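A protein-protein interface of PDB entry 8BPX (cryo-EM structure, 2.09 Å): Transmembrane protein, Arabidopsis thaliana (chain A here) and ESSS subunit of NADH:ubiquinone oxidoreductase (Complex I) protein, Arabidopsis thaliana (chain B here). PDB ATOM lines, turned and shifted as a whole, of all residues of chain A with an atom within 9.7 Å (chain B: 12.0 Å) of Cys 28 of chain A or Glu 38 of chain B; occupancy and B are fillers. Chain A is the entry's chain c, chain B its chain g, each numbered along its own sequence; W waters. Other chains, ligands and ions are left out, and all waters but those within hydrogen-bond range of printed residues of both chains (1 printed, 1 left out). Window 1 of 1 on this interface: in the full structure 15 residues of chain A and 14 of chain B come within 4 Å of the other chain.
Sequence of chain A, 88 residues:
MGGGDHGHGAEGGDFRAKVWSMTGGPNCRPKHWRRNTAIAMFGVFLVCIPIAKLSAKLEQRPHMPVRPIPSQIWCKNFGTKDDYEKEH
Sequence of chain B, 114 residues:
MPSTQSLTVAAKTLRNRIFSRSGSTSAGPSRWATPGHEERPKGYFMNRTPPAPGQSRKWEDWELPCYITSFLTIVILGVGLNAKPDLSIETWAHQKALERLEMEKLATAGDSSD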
ATOM      1  N   ARG A  16     -14.867   5.263  28.173  1.00  0.00           N
ATOM      2  CA  ARG A  16     -14.314   6.369  27.402  1.00  0.00           C
ATOM      3  C   ARG A  16     -14.661   7.731  27.997  1.00  0.00           C
ATOM      4  O   ARG A  16     -13.984   8.718  27.695  1.00  0.00           O
ATOM      5  CB  ARG A  16     -14.786   6.271  25.951  1.00  0.00           C
ATOM      6  CG  ARG A  16     -14.096   5.153  25.161  1.00  0.00           C
ATOM      7  CD  ARG A  16     -14.522   5.125  23.701  1.00  0.00           C
ATOM      8  NE  ARG A  16     -15.943   4.849  23.550  1.00  0.00           N
ATOM      9  CZ  ARG A  16     -16.541   4.564  22.401  1.00  0.00           C
ATOM     10  NH1 ARG A  16     -15.868   4.505  21.266  1.00  0.00           N
ATOM     11  NH2 ARG A  16     -17.849   4.336  22.391  1.00  0.00           N
ATOM     12  N   ALA A  17     -15.688   7.805  28.845  1.00  0.00           N
ATOM     13  CA  ALA A  17     -15.999   9.035  29.561  1.00  0.00           C
ATOM     14  C   ALA A  17     -14.934   9.402  30.584  1.00  0.00           C
ATOM     15  O   ALA A  17     -14.931  10.533  31.071  1.00  0.00           O
ATOM     16  CB  ALA A  17     -17.353   8.910  30.256  1.00  0.00           C
ATOM     17  N   LYS A  18     -14.042   8.480  30.926  1.00  0.00           N
ATOM     18  CA  LYS A  18     -12.945   8.764  31.832  1.00  0.00           C
ATOM     19  C   LYS A  18     -11.625   8.962  31.103  1.00  0.00           C
ATOM     20  O   LYS A  18     -10.577   9.031  31.750  1.00  0.00           O
ATOM     21  CB  LYS A  18     -12.815   7.641  32.862  1.00  0.00           C
ATOM     22  CG  LYS A  18     -14.137   7.220  33.468  1.00  0.00           C
ATOM     23  CD  LYS A  18     -14.020   5.884  34.164  1.00  0.00           C
ATOM     24  CE  LYS A  18     -13.490   6.045  35.576  1.00  0.00           C
ATOM     25  NZ  LYS A  18     -12.013   6.001  35.639  1.00  0.00           N
ATOM     26  N   VAL A  19     -11.649   9.056  29.779  1.00  0.00           N
ATOM     27  CA  VAL A  19     -10.435   9.114  28.976  1.00  0.00           C
ATOM     28  C   VAL A  19     -10.336  10.507  28.368  1.00  0.00           C
ATOM     29  O   VAL A  19     -11.217  10.929  27.611  1.00  0.00           O
ATOM     30  CB  VAL A  19     -10.425   8.029  27.888  1.00  0.00           C
ATOM     31  CG1 VAL A  19      -9.367   8.333  26.836  1.00  0.00           C
ATOM     32  CG2 VAL A  19     -10.223   6.649  28.506  1.00  0.00           C
ATOM     33  N   SER A  21      -8.779  13.278  25.894  1.00  0.00           N
ATOM     34  CA  SER A  21      -8.079  13.453  24.628  1.00  0.00           C
ATOM     35  C   SER A  21      -8.165  14.911  24.198  1.00  0.00           C
ATOM     36  O   SER A  21      -9.039  15.661  24.635  1.00  0.00           O
ATOM     37  CB  SER A  21      -8.632  12.547  23.514  1.00  0.00           C
ATOM     38  OG  SER A  21     -10.024  12.701  23.351  1.00  0.00           O
ATOM     39  N   MET A  22      -7.233  15.307  23.328  1.00  0.00           N
ATOM     40  CA  MET A  22      -7.229  16.670  22.810  1.00  0.00           C
ATOM     41  C   MET A  22      -8.379  16.909  21.838  1.00  0.00           C
ATOM     42  O   MET A  22      -8.939  18.008  21.790  1.00  0.00           O
ATOM     43  CB  MET A  22      -5.893  16.976  22.132  1.00  0.00           C
ATOM     44  CG  MET A  22      -4.750  17.255  23.083  1.00  0.00           C
ATOM     45  SD  MET A  22      -3.192  17.528  22.214  1.00  0.00           S
ATOM     46  CE  MET A  22      -3.335  16.348  20.883  1.00  0.00           C
ATOM     47  N   THR A  23      -8.739  15.899  21.050  1.00  0.00           N
ATOM     48  CA  THR A  23      -9.809  16.046  20.074  1.00  0.00           C
ATOM     49  C   THR A  23     -11.187  15.838  20.691  1.00  0.00           C
ATOM     50  O   THR A  23     -12.194  16.113  20.031  1.00  0.00           O
ATOM     51  CB  THR A  23      -9.581  15.076  18.911  1.00  0.00           C
ATOM     52  OG1 THR A  23      -8.183  15.029  18.606  1.00  0.00           O
ATOM     53  CG2 THR A  23     -10.312  15.539  17.662  1.00  0.00           C
ATOM     54  N   GLY A  24     -11.255  15.375  21.937  1.00  0.00           N
ATOM     55  CA  GLY A  24     -12.494  15.327  22.677  1.00  0.00           C
ATOM     56  C   GLY A  24     -13.144  13.965  22.801  1.00  0.00           C
ATOM     57  O   GLY A  24     -14.103  13.836  23.564  1.00  0.00           O
ATOM     58  N   GLY A  25     -12.674  12.957  22.078  1.00  0.00           N
ATOM     59  CA  GLY A  25     -13.254  11.637  22.167  1.00  0.00           C
ATOM     60  C   GLY A  25     -14.598  11.526  21.472  1.00  0.00           C
ATOM     61  O   GLY A  25     -15.009  12.414  20.725  1.00  0.00           O
ATOM     62  N   PRO A  26     -15.314  10.431  21.718  1.00  0.00           N
ATOM     63  CA  PRO A  26     -16.550  10.166  20.972  1.00  0.00           C
ATOM     64  C   PRO A  26     -17.730  11.013  21.432  1.00  0.00           C
ATOM     65  O   PRO A  26     -17.976  11.175  22.630  1.00  0.00           O
ATOM     66  CB  PRO A  26     -16.806   8.679  21.244  1.00  0.00           C
ATOM     67  CG  PRO A  26     -16.174   8.437  22.572  1.00  0.00           C
ATOM     68  CD  PRO A  26     -14.981   9.338  22.650  1.00  0.00           C
ATOM     69  N   ASN A  27     -18.473  11.534  20.452  1.00  0.00           N
ATOM     70  CA  ASN A  27     -19.720  12.268  20.686  1.00  0.00           C
ATOM     71  C   ASN A  27     -19.500  13.469  21.605  1.00  0.00           C
ATOM     72  O   ASN A  27     -20.212  13.666  22.587  1.00  0.00           O
ATOM     73  CB  ASN A  27     -20.802  11.342  21.246  1.00  0.00           C
ATOM     74  CG  ASN A  27     -21.177  10.234  20.285  1.00  0.00           C
ATOM     75  OD1 ASN A  27     -21.572  10.488  19.153  1.00  0.00           O
ATOM     76  ND2 ASN A  27     -21.026   8.995  20.727  1.00  0.00           N
ATOM     77  N   CYS A  28     -18.498  14.277  21.274  1.00  0.00           N
ATOM     78  CA  CYS A  28     -18.112  15.404  22.114  1.00  0.00           C
ATOM     79  C   CYS A  28     -19.079  16.570  21.908  1.00  0.00           C
ATOM     80  O   CYS A  28     -19.205  17.092  20.795  1.00  0.00           O
ATOM     81  CB  CYS A  28     -16.677  15.822  21.805  1.00  0.00           C
ATOM     82  SG  CYS A  28     -16.027  17.120  22.870  1.00  0.00           S
ATOM     83  N   ARG A  29     -19.749  16.975  22.984  1.00  0.00           N
ATOM     84  CA  ARG A  29     -20.755  18.039  22.970  1.00  0.00           C
ATOM     85  C   ARG A  29     -20.480  19.018  24.103  1.00  0.00           C
ATOM     86  O   ARG A  29     -21.237  19.072  25.077  1.00  0.00           O
ATOM     87  CB  ARG A  29     -22.155  17.450  23.139  1.00  0.00           C
ATOM     88  CG  ARG A  29     -22.609  16.505  22.053  1.00  0.00           C
ATOM     89  CD  ARG A  29     -23.086  17.247  20.830  1.00  0.00           C
ATOM     90  NE  ARG A  29     -24.081  18.238  21.216  1.00  0.00           N
ATOM     91  CZ  ARG A  29     -24.713  19.041  20.374  1.00  0.00           C
ATOM     92  NH1 ARG A  29     -24.613  18.884  19.068  1.00  0.00           N
ATOM     93  NH2 ARG A  29     -25.500  19.996  20.857  1.00  0.00           N
ATOM     94  N   PRO A  30     -19.412  19.812  24.014  1.00  0.00           N
ATOM     95  CA  PRO A  30     -19.145  20.790  25.076  1.00  0.00           C
ATOM     96  C   PRO A  30     -20.289  21.788  25.209  1.00  0.00           C
ATOM     97  O   PRO A  30     -20.883  22.218  24.218  1.00  0.00           O
ATOM     98  CB  PRO A  30     -17.843  21.465  24.625  1.00  0.00           C
ATOM     99  CG  PRO A  30     -17.717  21.148  23.187  1.00  0.00           C
ATOM    100  CD  PRO A  30     -18.384  19.842  22.964  1.00  0.00           C
ATOM    101  N   LYS A  31     -20.592  22.152  26.457  1.00  0.00           N
ATOM    102  CA  LYS A  31     -21.762  22.979  26.731  1.00  0.00           C
ATOM    103  C   LYS A  31     -21.616  24.374  26.136  1.00  0.00           C
ATOM    104  O   LYS A  31     -22.585  24.939  25.617  1.00  0.00           O
ATOM    105  CB  LYS A  31     -22.006  23.058  28.239  1.00  0.00           C
ATOM    106  CG  LYS A  31     -22.882  24.213  28.669  1.00  0.00           C
ATOM    107  CD  LYS A  31     -22.503  24.706  30.052  1.00  0.00           C
ATOM    108  CE  LYS A  31     -23.660  24.550  31.029  1.00  0.00           C
ATOM    109  NZ  LYS A  31     -23.513  25.432  32.222  1.00  0.00           N
ATOM    110  N   HIS A  32     -20.414  24.937  26.189  1.00  0.00           N
ATOM    111  CA  HIS A  32     -20.154  26.290  25.704  1.00  0.00           C
ATOM    112  C   HIS A  32     -19.488  26.289  24.338  1.00  0.00           C
ATOM    113  O   HIS A  32     -18.643  27.139  24.053  1.00  0.00           O
ATOM    114  CB  HIS A  32     -19.306  27.048  26.714  1.00  0.00           C
ATOM    115  CG  HIS A  32     -19.995  27.272  28.023  1.00  0.00           C
ATOM    116  ND1 HIS A  32     -21.219  27.896  28.117  1.00  0.00           N
ATOM    117  CD2 HIS A  32     -19.638  26.944  29.286  1.00  0.00           C
ATOM    118  CE1 HIS A  32     -21.582  27.952  29.386  1.00  0.00           C
ATOM    119  NE2 HIS A  32     -20.638  27.384  30.116  1.00  0.00           N
ATOM    120  N   TRP A  33     -19.865  25.351  23.468  1.00  0.00           N
ATOM    121  CA  TRP A  33     -19.133  25.173  22.219  1.00  0.00           C
ATOM    122  C   TRP A  33     -19.288  26.365  21.279  1.00  0.00           C
ATOM    123  O   TRP A  33     -18.390  26.623  20.477  1.00  0.00           O
ATOM    124  CB  TRP A  33     -19.566  23.878  21.527  1.00  0.00           C
ATOM    125  CG  TRP A  33     -20.928  23.918  20.922  1.00  0.00           C
ATOM    126  CD1 TRP A  33     -22.090  23.502  21.493  1.00  0.00           C
ATOM    127  CD2 TRP A  33     -21.272  24.392  19.615  1.00  0.00           C
ATOM    128  NE1 TRP A  33     -23.137  23.690  20.629  1.00  0.00           N
ATOM    129  CE2 TRP A  33     -22.662  24.235  19.468  1.00  0.00           C
ATOM    130  CE3 TRP A  33     -20.538  24.935  18.557  1.00  0.00           C
ATOM    131  CZ2 TRP A  33     -23.336  24.602  18.306  1.00  0.00           C
ATOM    132  CZ3 TRP A  33     -21.208  25.298  17.405  1.00  0.00           C
ATOM    133  CH2 TRP A  33     -22.591  25.131  17.288  1.00  0.00           C
ATOM    134  N   ARG A  35     -19.519  29.732  22.155  1.00  0.00           N
ATOM    135  CA  ARG A  35     -18.579  30.756  22.589  1.00  0.00           C
ATOM    136  C   ARG A  35     -17.141  30.312  22.337  1.00  0.00           C
ATOM    137  O   ARG A  35     -16.292  31.117  21.941  1.00  0.00           O
ATOM    138  CB  ARG A  35     -18.812  31.083  24.064  1.00  0.00           C
ATOM    139  CG  ARG A  35     -17.610  31.665  24.779  1.00  0.00           C
ATOM    140  CD  ARG A  35     -17.617  31.314  26.247  1.00  0.00           C
ATOM    141  NE  ARG A  35     -16.826  30.121  26.515  1.00  0.00           N
ATOM    142  CZ  ARG A  35     -16.824  29.465  27.667  1.00  0.00           C
ATOM    143  NH1 ARG A  35     -17.556  29.867  28.691  1.00  0.00           N
ATOM    144  NH2 ARG A  35     -16.073  28.375  27.791  1.00  0.00           N
ATOM    145  N   ASN A  36     -16.859  29.023  22.533  1.00  0.00           N
ATOM    146  CA  ASN A  36     -15.520  28.511  22.264  1.00  0.00           C
ATOM    147  C   ASN A  36     -15.181  28.587  20.780  1.00  0.00           C
ATOM    148  O   ASN A  36     -14.046  28.909  20.413  1.00  0.00           O
ATOM    149  CB  ASN A  36     -15.401  27.083  22.790  1.00  0.00           C
ATOM    150  CG  ASN A  36     -15.520  27.014  24.297  1.00  0.00           C
ATOM    151  OD1 ASN A  36     -15.332  28.014  24.983  1.00  0.00           O
ATOM    152  ND2 ASN A  36     -15.836  25.841  24.818  1.00  0.00           N
ATOM    153  N   SER B  30     -30.951  20.981  15.338  1.00  0.00           N
ATOM    154  CA  SER B  30     -30.984  21.115  16.789  1.00  0.00           C
ATOM    155  C   SER B  30     -29.577  21.027  17.367  1.00  0.00           C
ATOM    156  O   SER B  30     -29.310  21.547  18.449  1.00  0.00           O
ATOM    157  CB  SER B  30     -31.879  20.042  17.410  1.00  0.00           C
ATOM    158  OG  SER B  30     -31.332  18.748  17.220  1.00  0.00           O
ATOM    159  N   ARG B  31     -28.677  20.371  16.632  1.00  0.00           N
ATOM    160  CA  ARG B  31     -27.286  20.278  17.051  1.00  0.00           C
ATOM    161  C   ARG B  31     -26.582  21.625  17.032  1.00  0.00           C
ATOM    162  O   ARG B  31     -25.496  21.747  17.606  1.00  0.00           O
ATOM    163  CB  ARG B  31     -26.525  19.294  16.157  1.00  0.00           C
ATOM    164  CG  ARG B  31     -26.274  19.818  14.755  1.00  0.00           C
ATOM    165  CD  ARG B  31     -25.480  18.845  13.890  1.00  0.00           C
ATOM    166  NE  ARG B  31     -24.052  19.146  13.888  1.00  0.00           N
ATOM    167  CZ  ARG B  31     -23.137  18.454  13.224  1.00  0.00           C
ATOM    168  NH1 ARG B  31     -23.469  17.454  12.424  1.00  0.00           N
ATOM    169  NH2 ARG B  31     -21.856  18.782  13.355  1.00  0.00           N
ATOM    170  N   TRP B  32     -27.166  22.637  16.385  1.00  0.00           N
ATOM    171  CA  TRP B  32     -26.556  23.956  16.318  1.00  0.00           C
ATOM    172  C   TRP B  32     -27.205  24.976  17.241  1.00  0.00           C
ATOM    173  O   TRP B  32     -26.572  25.990  17.551  1.00  0.00           O
ATOM    174  CB  TRP B  32     -26.597  24.494  14.880  1.00  0.00           C
ATOM    175  CG  TRP B  32     -26.123  23.513  13.862  1.00  0.00           C
ATOM    176  CD1 TRP B  32     -26.893  22.700  13.096  1.00  0.00           C
ATOM    177  CD2 TRP B  32     -24.765  23.233  13.507  1.00  0.00           C
ATOM    178  NE1 TRP B  32     -26.106  21.932  12.277  1.00  0.00           N
ATOM    179  CE2 TRP B  32     -24.793  22.238  12.512  1.00  0.00           C
ATOM    180  CE3 TRP B  32     -23.530  23.731  13.926  1.00  0.00           C
ATOM    181  CZ2 TRP B  32     -23.632  21.727  11.934  1.00  0.00           C
ATOM    182  CZ3 TRP B  32     -22.379  23.222  13.349  1.00  0.00           C
ATOM    183  CH2 TRP B  32     -22.438  22.227  12.369  1.00  0.00           C
ATOM    184  N   THR B  34     -29.084  23.999  20.295  1.00  0.00           N
ATOM    185  CA  THR B  34     -29.227  23.508  21.656  1.00  0.00           C
ATOM    186  C   THR B  34     -27.856  23.173  22.227  1.00  0.00           C
ATOM    187  O   THR B  34     -27.133  22.351  21.647  1.00  0.00           O
ATOM    188  CB  THR B  34     -30.129  22.264  21.707  1.00  0.00           C
ATOM    189  OG1 THR B  34     -29.802  21.387  20.624  1.00  0.00           O
ATOM    190  CG2 THR B  34     -31.594  22.666  21.606  1.00  0.00           C
ATOM    191  N   PRO B  35     -27.462  23.779  23.345  1.00  0.00           N
ATOM    192  CA  PRO B  35     -26.085  23.626  23.826  1.00  0.00           C
ATOM    193  C   PRO B  35     -25.786  22.200  24.262  1.00  0.00           C
ATOM    194  O   PRO B  35     -26.680  21.403  24.559  1.00  0.00           O
ATOM    195  CB  PRO B  35     -26.014  24.595  25.009  1.00  0.00           C
ATOM    196  CG  PRO B  35     -27.420  24.698  25.496  1.00  0.00           C
ATOM    197  CD  PRO B  35     -28.312  24.513  24.299  1.00  0.00           C
ATOM    198  N   GLY B  36     -24.493  21.888  24.295  1.00  0.00           N
ATOM    199  CA  GLY B  36     -24.049  20.550  24.617  1.00  0.00           C
ATOM    200  C   GLY B  36     -24.263  20.192  26.074  1.00  0.00           C
ATOM    201  O   GLY B  36     -24.594  21.021  26.921  1.00  0.00           O
ATOM    202  N   HIS B  37     -24.058  18.908  26.369  1.00  0.00           N
ATOM    203  CA  HIS B  37     -24.352  18.362  27.688  1.00  0.00           C
ATOM    204  C   HIS B  37     -23.124  18.174  28.568  1.00  0.00           C
ATOM    205  O   HIS B  37     -23.275  18.015  29.783  1.00  0.00           O
ATOM    206  CB  HIS B  37     -25.084  17.019  27.552  1.00  0.00           C
ATOM    207  CG  HIS B  37     -24.349  16.008  26.726  1.00  0.00           C
ATOM    208  ND1 HIS B  37     -23.107  15.520  27.071  1.00  0.00           N
ATOM    209  CD2 HIS B  37     -24.691  15.385  25.572  1.00  0.00           C
ATOM    210  CE1 HIS B  37     -22.712  14.644  26.164  1.00  0.00           C
ATOM    211  NE2 HIS B  37     -23.655  14.544  25.244  1.00  0.00           N
ATOM    212  N   GLU B  38     -21.924  18.186  27.998  1.00  0.00           N
ATOM    213  CA  GLU B  38     -20.704  18.013  28.784  1.00  0.00           C
ATOM    214  C   GLU B  38     -20.438  19.293  29.566  1.00  0.00           C
ATOM    215  O   GLU B  38     -19.832  20.236  29.051  1.00  0.00           O
ATOM    216  CB  GLU B  38     -19.524  17.666  27.882  1.00  0.00           C
ATOM    217  CG  GLU B  38     -19.882  16.826  26.669  1.00  0.00           C
ATOM    218  CD  GLU B  38     -18.680  16.501  25.800  1.00  0.00           C
ATOM    219  OE1 GLU B  38     -18.037  17.430  25.271  1.00  0.00           O
ATOM    220  OE2 GLU B  38     -18.389  15.299  25.626  1.00  0.00           O
ATOM    221  N   GLU B  39     -20.904  19.337  30.817  1.00  0.00           N
ATOM    222  CA  GLU B  39     -20.589  20.472  31.678  1.00  0.00           C
ATOM    223  C   GLU B  39     -19.091  20.555  31.924  1.00  0.00           C
ATOM    224  O   GLU B  39     -18.509  21.647  31.916  1.00  0.00           O
ATOM    225  CB  GLU B  39     -21.340  20.362  33.006  1.00  0.00           C
ATOM    226  CG  GLU B  39     -22.784  19.902  32.890  1.00  0.00           C
ATOM    227  CD  GLU B  39     -22.915  18.391  32.880  1.00  0.00           C
ATOM    228  OE1 GLU B  39     -21.894  17.707  33.109  1.00  0.00           O
ATOM    229  OE2 GLU B  39     -24.034  17.886  32.645  1.00  0.00           O
ATOM    230  N   ARG B  40     -18.454  19.411  32.136  1.00  0.00           N
ATOM    231  CA  ARG B  40     -17.012  19.287  32.228  1.00  0.00           C
ATOM    232  C   ARG B  40     -16.561  18.219  31.245  1.00  0.00           C
ATOM    233  O   ARG B  40     -17.323  17.303  30.925  1.00  0.00           O
ATOM    234  CB  ARG B  40     -16.562  18.919  33.650  1.00  0.00           C
ATOM    235  CG  ARG B  40     -16.796  19.993  34.709  1.00  0.00           C
ATOM    236  CD  ARG B  40     -16.285  19.583  36.081  1.00  0.00           C
ATOM    237  NE  ARG B  40     -16.582  20.592  37.090  1.00  0.00           N
ATOM    238  CZ  ARG B  40     -16.353  20.446  38.388  1.00  0.00           C
ATOM    239  NH1 ARG B  40     -15.798  19.348  38.872  1.00  0.00           N
ATOM    240  NH2 ARG B  40     -16.685  21.430  39.219  1.00  0.00           N
ATOM    241  N   PRO B  41     -15.338  18.321  30.737  1.00  0.00           N
ATOM    242  CA  PRO B  41     -14.875  17.356  29.734  1.00  0.00           C
ATOM    243  C   PRO B  41     -14.739  15.952  30.309  1.00  0.00           C
ATOM    244  O   PRO B  41     -14.743  15.739  31.523  1.00  0.00           O
ATOM    245  CB  PRO B  41     -13.513  17.915  29.313  1.00  0.00           C
ATOM    246  CG  PRO B  41     -13.544  19.358  29.697  1.00  0.00           C
ATOM    247  CD  PRO B  41     -14.375  19.415  30.938  1.00  0.00           C
ATOM    248  N   LYS B  42     -14.597  14.995  29.383  1.00  0.00           N
ATOM    249  CA  LYS B  42     -14.397  13.581  29.789  1.00  0.00           C
ATOM    250  C   LYS B  42     -12.906  13.368  30.062  1.00  0.00           C
ATOM    251  O   LYS B  42     -12.079  13.878  29.279  1.00  0.00           O
ATOM    252  CB  LYS B  42     -14.949  12.634  28.716  1.00  0.00           C
ATOM    253  CG  LYS B  42     -14.482  12.887  27.289  1.00  0.00           C
ATOM    254  CD  LYS B  42     -14.768  11.744  26.340  1.00  0.00           C
ATOM    255  CE  LYS B  42     -16.210  11.663  25.887  1.00  0.00           C
ATOM    256  NZ  LYS B  42     -16.564  12.784  24.983  1.00  0.00           N
ATOM    257  N   GLY B  43     -12.580  12.654  31.138  1.00  0.00           N
ATOM    258  CA  GLY B  43     -11.210  12.422  31.539  1.00  0.00           C
ATOM    259  C   GLY B  43     -10.616  13.580  32.320  1.00  0.00           C
ATOM    260  O   GLY B  43     -11.242  14.609  32.568  1.00  0.00           O
ATOM    261  N   TYR B  44      -9.364  13.394  32.716  1.00  0.00           N
ATOM    262  CA  TYR B  44      -8.590  14.434  33.374  1.00  0.00           C
ATOM    263  C   TYR B  44      -7.270  14.563  32.643  1.00  0.00           C
ATOM    264  O   TYR B  44      -6.643  13.551  32.318  1.00  0.00           O
ATOM    265  CB  TYR B  44      -8.356  14.109  34.850  1.00  0.00           C
ATOM    266  CG  TYR B  44      -9.595  14.305  35.677  1.00  0.00           C
ATOM    267  CD1 TYR B  44     -10.224  15.536  35.728  1.00  0.00           C
ATOM    268  CD2 TYR B  44     -10.153  13.251  36.384  1.00  0.00           C
ATOM    269  CE1 TYR B  44     -11.365  15.718  36.461  1.00  0.00           C
ATOM    270  CE2 TYR B  44     -11.297  13.426  37.132  1.00  0.00           C
ATOM    271  CZ  TYR B  44     -11.897  14.662  37.166  1.00  0.00           C
ATOM    272  OH  TYR B  44     -13.039  14.852  37.908  1.00  0.00           O
HETATM  273  O   HOH W   1      -7.948  10.849  32.039  1.00  0.00           O
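The backbone NH (N) of Gly 43 of chain B sits at hydrogen-bond distance from the backbone carbonyl oxygen (O) of Ala 17 of chain A, at 3.2 Å. The side-chain amino group (NZ) of Lys 42 of chain B lies within hydrogen-bond range of the backbone carbonyl oxygen (O) of Gly 24 of chain A, 3.0 Å away. O of Pro 26 of chain A lies within hydrogen-bond range of NZ of Lys 42 of chain B (3.2 Å). SG of Cys 28 of chain A lies within hydrogen-bond range of OE1 of Glu 38 of chain B (3.1 Å). NH1 of Arg 29 of chain A lies within hydrogen-bond range of O of Arg 31 of chain B. The backbone carbonyl oxygen of Thr 34 of chain B is in hydrogen-bond range of the guanidinium group of Arg 29 of chain A, 3.0 Å away. The backbone NH (N) of His 37 of chain B sits at hydrogen-bond distance from the backbone carbonyl oxygen (O) of Arg 29 of chain A, 3.1 Å away. The backbone NH of Arg 29 of chain A is in hydrogen-bond range of the side-chain carboxylate of Glu 38 of chain B. N of Lys 31 of chain A sits at hydrogen-bond distance from O of Glu 38 of chain B (3.3 Å). O of Lys 42 of chain B sits close to O of Val 19 of chain A. The backbone nitrogen of Pro 30 of chain A sits close to the side-chain carboxylate of Glu 38 of chain B (3.0 Å).
OG of Ser 21 of chain A lies within hydrogen-bond range of N of Gly 24 of chain A (3.3 Å). The side-chain amino group (NZ) of Lys 42 of chain B lies within salt-bridge range of the side-chain carboxylate (OE2) of Glu 38 of chain B (3.2 Å).
Among the printed residues, merely in contact across the chains: Arg 16 of chain A with Lys 42 of chain B (3.4 Å), Ala 17 of chain A with Lys 42 of chain B (3.2 Å), Lys 18 of chain A with Gly 43 of chain B (3.5 Å), Val 19 of chain A with Gly 43 of chain B (3.8 Å), Asn 27 of chain A with Glu 38 of chain B (3.9 Å), Arg 29 of chain A with Gly 36 of chain B (3.2 Å), Pro 30 of chain A with Gly 36 of chain B (3.6 Å), Lys 31 of chain A with Pro 35 of chain B (3.5 Å), Lys 31 of chain A with Gly 36 of chain B (3.4 Å), Trp 33 of chain A with Arg 31 of chain B (3.6 Å) and Trp 33 of chain A with Trp 32 of chain B (3.6 Å).
Of the printed residues of chain B, Ala 17 of chain A touches Lys 42 (3.2 Å) and Gly 43 (3.2 Å). Of chain B, only Lys 42 comes within 4 Å of Gly 24 of chain A. No residue of chain B comes within 4 Å of Gly 25 of chain A. Of chain B, only Lys 42 comes within 4 Å of Pro 26 of chain A. Of chain B, only Glu 38 (3.9 Å) comes within 4 Å of Asn 27 of chain A. Cys 28 of chain A touches just one residue of chain B: Glu 38 (3.1 Å). Arg 29 of chain A touches just these residues of chain B: Arg 31, Thr 34, Gly 36, His 37 and Glu 38. Of chain B, only Gly 36 (3.6 Å) and Glu 38 (3.0 Å) come within 4 Å of Pro 30 of chain A. Of chain B, only Pro 35 (3.5 Å), Gly 36 (3.4 Å) and Glu 38 (3.3 Å) come within 4 Å of Lys 31 of chain A. Printed residues of chain B within 4 Å of Trp 33 of chain A: Arg 31 (3.6 Å) and Trp 32 (3.6 Å). Printed residues of chain A within 4 Å of Thr 34 of chain B: Arg 29. Of the printed residues of chain A, His 37 of chain B touches Arg 29 (3.1 Å). Glu 38 of chain B touches just these residues of chain A: Asn 27, Cys 28, Arg 29, Pro 30 and Lys 31. No residue of chain A comes within 4 Å of Glu 39 of chain B. Of the printed residues of chain A, Lys 42 of chain B touches Arg 16, Ala 17, Val 19, Gly 24 and Pro 26. The nearest residue of chain B that does not touch Cys 28 of chain A is Lys 42 of chain B (4.2 Å). The nearest residue of chain A that does not touch Glu 38 of chain B is Gly 24 of chain A (5.0 Å). The nearest printed residue of chain A that does not touch Pro 35 of chain B is Arg 29 of chain A (4.1 Å).
Printed residues of chain A that touch a printed residue of chain B: Arg 16, Ala 17, Lys 18, Val 19, Gly 24, Pro 26, Asn 27, Cys 28, Arg 29, Pro 30, Lys 31 and Trp 33. Hydrophobic or aromatic side chains of chain A that line the printed part of chain B: Pro 30 and Trp 33. Along chain A the printed residues that touch a printed residue of chain B span positions 16 to 33. Of the 14 printed residues of chain B, 9 touch a printed residue of chain A. Hydrophobic or aromatic side chains of chain B within 4 Å of the printed part of chain A: Trp 32, Pro 35 and His 37. Among the printed residues, 22 pairs touch across the chains. Among the printed residues, no Asp or Glu carboxylate lies within 4 Å of a Lys or Arg side-chain nitrogen of the other chain.
Water W1 lies within hydrogen-bond range of the backbone NH of Tyr 44 of chain B (3.0 Å) and the backbone carbonyl oxygen of Lys 18 of chain A (3.2 Å).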
